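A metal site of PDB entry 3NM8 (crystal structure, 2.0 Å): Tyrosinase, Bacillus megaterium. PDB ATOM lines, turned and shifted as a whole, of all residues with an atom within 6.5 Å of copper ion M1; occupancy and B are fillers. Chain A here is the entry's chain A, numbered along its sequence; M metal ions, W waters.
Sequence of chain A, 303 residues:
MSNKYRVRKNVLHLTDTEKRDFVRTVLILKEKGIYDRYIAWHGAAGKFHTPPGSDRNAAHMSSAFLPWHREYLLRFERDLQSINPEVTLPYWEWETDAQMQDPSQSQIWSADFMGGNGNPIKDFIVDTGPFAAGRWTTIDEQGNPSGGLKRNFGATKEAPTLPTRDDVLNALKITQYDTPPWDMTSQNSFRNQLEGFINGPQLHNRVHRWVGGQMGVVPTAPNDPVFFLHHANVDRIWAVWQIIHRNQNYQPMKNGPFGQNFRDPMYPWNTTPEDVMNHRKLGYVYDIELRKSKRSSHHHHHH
ND1 of His 204 sits at hydrogen-bond distance from ND2 of Asn 205 (2.8 Å).
Copper ion M1 is bound by NE2 of His 231, NE2 of His 204, NE2 of His 208 and water W1.
Phe 227 touches copper ion M1 (CE2 to CU, 3.9 Å).
Four residues have an atom within 4 Å of copper ion M1: His 204, His 208, Phe 227 and His 231.
The nearest printed residue that does not touch copper ion M1 is His 69 (4.2 Å).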
ATOM      1  N   HIS A  42      -4.388 -36.501 -10.534  1.00  0.00           N
ATOM      2  CA  HIS A  42      -4.770 -35.543 -11.560  1.00  0.00           C
ATOM      3  C   HIS A  42      -5.195 -36.256 -12.838  1.00  0.00           C
ATOM      4  O   HIS A  42      -6.106 -35.814 -13.514  1.00  0.00           O
ATOM      5  CB  HIS A  42      -3.589 -34.605 -11.810  1.00  0.00           C
ATOM      6  CG  HIS A  42      -3.801 -33.670 -12.963  1.00  0.00           C
ATOM      7  ND1 HIS A  42      -3.448 -33.997 -14.247  1.00  0.00           N
ATOM      8  CD2 HIS A  42      -4.277 -32.412 -13.007  1.00  0.00           C
ATOM      9  CE1 HIS A  42      -3.699 -32.972 -15.046  1.00  0.00           C
ATOM     10  NE2 HIS A  42      -4.208 -31.998 -14.312  1.00  0.00           N
ATOM     11  N   HIS A  60     -11.321 -30.437 -14.501  1.00  0.00           N
ATOM     12  CA  HIS A  60     -11.305 -29.408 -15.540  1.00  0.00           C
ATOM     13  C   HIS A  60     -12.638 -29.225 -16.249  1.00  0.00           C
ATOM     14  O   HIS A  60     -13.576 -30.011 -16.064  1.00  0.00           O
ATOM     15  CB  HIS A  60     -10.296 -29.725 -16.637  1.00  0.00           C
ATOM     16  CG  HIS A  60      -8.985 -30.239 -16.152  1.00  0.00           C
ATOM     17  ND1 HIS A  60      -8.834 -31.510 -15.621  1.00  0.00           N
ATOM     18  CD2 HIS A  60      -7.755 -29.680 -16.160  1.00  0.00           C
ATOM     19  CE1 HIS A  60      -7.562 -31.712 -15.335  1.00  0.00           C
ATOM     20  NE2 HIS A  60      -6.886 -30.623 -15.650  1.00  0.00           N
ATOM     21  N   PHE A  65     -12.920 -26.841 -11.278  1.00  0.00           N
ATOM     22  CA  PHE A  65     -11.544 -26.624 -11.720  1.00  0.00           C
ATOM     23  C   PHE A  65     -10.688 -25.898 -10.678  1.00  0.00           C
ATOM     24  O   PHE A  65      -9.611 -26.371 -10.318  1.00  0.00           O
ATOM     25  CB  PHE A  65     -11.546 -25.816 -13.019  1.00  0.00           C
ATOM     26  CG  PHE A  65     -10.200 -25.285 -13.410  1.00  0.00           C
ATOM     27  CD1 PHE A  65      -9.161 -26.161 -13.714  1.00  0.00           C
ATOM     28  CD2 PHE A  65      -9.963 -23.914 -13.446  1.00  0.00           C
ATOM     29  CE1 PHE A  65      -7.895 -25.673 -14.062  1.00  0.00           C
ATOM     30  CE2 PHE A  65      -8.701 -23.411 -13.802  1.00  0.00           C
ATOM     31  CZ  PHE A  65      -7.669 -24.280 -14.104  1.00  0.00           C
ATOM     32  N   HIS A  69      -7.983 -27.765  -7.881  1.00  0.00           N
ATOM     33  CA  HIS A  69      -6.564 -27.549  -7.937  1.00  0.00           C
ATOM     34  C   HIS A  69      -6.041 -26.922  -6.673  1.00  0.00           C
ATOM     35  O   HIS A  69      -4.956 -27.110  -6.318  1.00  0.00           O
ATOM     36  CB  HIS A  69      -6.143 -26.768  -9.169  1.00  0.00           C
ATOM     37  CG  HIS A  69      -6.187 -27.564 -10.434  1.00  0.00           C
ATOM     38  ND1 HIS A  69      -7.308 -27.641 -11.216  1.00  0.00           N
ATOM     39  CD2 HIS A  69      -5.261 -28.322 -11.032  1.00  0.00           C
ATOM     40  CE1 HIS A  69      -7.060 -28.399 -12.243  1.00  0.00           C
ATOM     41  NE2 HIS A  69      -5.828 -28.820 -12.168  1.00  0.00           N
ATOM     42  N   HIS A 204      -4.267 -20.034 -18.095  1.00  0.00           N
ATOM     43  CA  HIS A 204      -3.896 -21.365 -17.657  1.00  0.00           C
ATOM     44  C   HIS A 204      -3.755 -22.305 -18.862  1.00  0.00           C
ATOM     45  O   HIS A 204      -2.649 -22.783 -19.140  1.00  0.00           O
ATOM     46  CB  HIS A 204      -4.939 -21.921 -16.690  1.00  0.00           C
ATOM     47  CG  HIS A 204      -4.916 -23.414 -16.563  1.00  0.00           C
ATOM     48  ND1 HIS A 204      -5.751 -24.233 -17.314  1.00  0.00           N
ATOM     49  CD2 HIS A 204      -4.182 -24.243 -15.785  1.00  0.00           C
ATOM     50  CE1 HIS A 204      -5.517 -25.497 -16.996  1.00  0.00           C
ATOM     51  NE2 HIS A 204      -4.568 -25.524 -16.074  1.00  0.00           N
ATOM     52  N   ASN A 205      -4.844 -22.557 -19.581  1.00  0.00           N
ATOM     53  CA  ASN A 205      -4.756 -23.395 -20.764  1.00  0.00           C
ATOM     54  C   ASN A 205      -3.611 -22.995 -21.678  1.00  0.00           C
ATOM     55  O   ASN A 205      -2.954 -23.845 -22.282  1.00  0.00           O
ATOM     56  CB  ASN A 205      -6.075 -23.369 -21.540  1.00  0.00           C
ATOM     57  CG  ASN A 205      -7.147 -24.227 -20.888  1.00  0.00           C
ATOM     58  OD1 ASN A 205      -8.289 -24.281 -21.368  1.00  0.00           O
ATOM     59  ND2 ASN A 205      -6.791 -24.901 -19.804  1.00  0.00           N
ATOM     60  N   HIS A 208      -0.094 -23.983 -20.216  1.00  0.00           N
ATOM     61  CA  HIS A 208       0.085 -25.404 -20.458  1.00  0.00           C
ATOM     62  C   HIS A 208       0.550 -25.606 -21.904  1.00  0.00           C
ATOM     63  O   HIS A 208       1.575 -26.232 -22.146  1.00  0.00           O
ATOM     64  CB  HIS A 208      -1.243 -26.155 -20.234  1.00  0.00           C
ATOM     65  CG  HIS A 208      -1.540 -26.470 -18.800  1.00  0.00           C
ATOM     66  ND1 HIS A 208      -0.873 -27.439 -18.083  1.00  0.00           N
ATOM     67  CD2 HIS A 208      -2.501 -25.995 -17.969  1.00  0.00           C
ATOM     68  CE1 HIS A 208      -1.399 -27.554 -16.890  1.00  0.00           C
ATOM     69  NE2 HIS A 208      -2.386 -26.681 -16.781  1.00  0.00           N
ATOM     70  N   ALA A 221       0.538 -33.841 -17.625  1.00  0.00           N
ATOM     71  CA  ALA A 221       1.011 -32.543 -17.141  1.00  0.00           C
ATOM     72  C   ALA A 221       1.832 -32.479 -15.839  1.00  0.00           C
ATOM     73  O   ALA A 221       2.951 -31.984 -15.837  1.00  0.00           O
ATOM     74  CB  ALA A 221      -0.156 -31.563 -17.064  1.00  0.00           C
ATOM     75  N   PHE A 227       4.301 -27.499 -13.108  1.00  0.00           N
ATOM     76  CA  PHE A 227       2.848 -27.610 -13.066  1.00  0.00           C
ATOM     77  C   PHE A 227       2.343 -26.979 -11.768  1.00  0.00           C
ATOM     78  O   PHE A 227       1.351 -26.254 -11.761  1.00  0.00           O
ATOM     79  CB  PHE A 227       2.410 -29.082 -13.132  1.00  0.00           C
ATOM     80  CG  PHE A 227       0.937 -29.309 -12.892  1.00  0.00           C
ATOM     81  CD1 PHE A 227       0.406 -29.268 -11.604  1.00  0.00           C
ATOM     82  CD2 PHE A 227       0.062 -29.530 -13.947  1.00  0.00           C
ATOM     83  CE1 PHE A 227      -0.962 -29.454 -11.372  1.00  0.00           C
ATOM     84  CE2 PHE A 227      -1.305 -29.721 -13.737  1.00  0.00           C
ATOM     85  CZ  PHE A 227      -1.822 -29.679 -12.453  1.00  0.00           C
ATOM     86  N   HIS A 230       2.825 -23.197 -11.775  1.00  0.00           N
ATOM     87  CA  HIS A 230       1.800 -22.631 -12.649  1.00  0.00           C
ATOM     88  C   HIS A 230       0.498 -22.482 -11.850  1.00  0.00           C
ATOM     89  O   HIS A 230      -0.054 -21.395 -11.671  1.00  0.00           O
ATOM     90  CB  HIS A 230       1.535 -23.556 -13.844  1.00  0.00           C
ATOM     91  CG  HIS A 230       0.421 -23.092 -14.739  1.00  0.00           C
ATOM     92  ND1 HIS A 230      -0.260 -23.938 -15.580  1.00  0.00           N
ATOM     93  CD2 HIS A 230      -0.118 -21.861 -14.922  1.00  0.00           C
ATOM     94  CE1 HIS A 230      -1.173 -23.255 -16.250  1.00  0.00           C
ATOM     95  NE2 HIS A 230      -1.111 -21.997 -15.862  1.00  0.00           N
ATOM     96  N   HIS A 231       0.004 -23.617 -11.384  1.00  0.00           N
ATOM     97  CA  HIS A 231      -1.224 -23.646 -10.629  1.00  0.00           C
ATOM     98  C   HIS A 231      -1.212 -22.855  -9.323  1.00  0.00           C
ATOM     99  O   HIS A 231      -2.265 -22.545  -8.789  1.00  0.00           O
ATOM    100  CB  HIS A 231      -1.654 -25.088 -10.444  1.00  0.00           C
ATOM    101  CG  HIS A 231      -2.436 -25.608 -11.610  1.00  0.00           C
ATOM    102  ND1 HIS A 231      -3.772 -25.305 -11.787  1.00  0.00           N
ATOM    103  CD2 HIS A 231      -2.045 -26.266 -12.728  1.00  0.00           C
ATOM    104  CE1 HIS A 231      -4.176 -25.763 -12.961  1.00  0.00           C
ATOM    105  NE2 HIS A 231      -3.144 -26.346 -13.558  1.00  0.00           N
HETATM  106 CU    CU M   1      -3.633 -27.049 -15.267  1.00  0.00          CU
HETATM  107 CU    CU M   2      -4.928 -30.371 -15.556  1.00  0.00          CU
HETATM  108  O   HOH W   1      -4.733 -28.507 -14.415  1.00  0.00           O
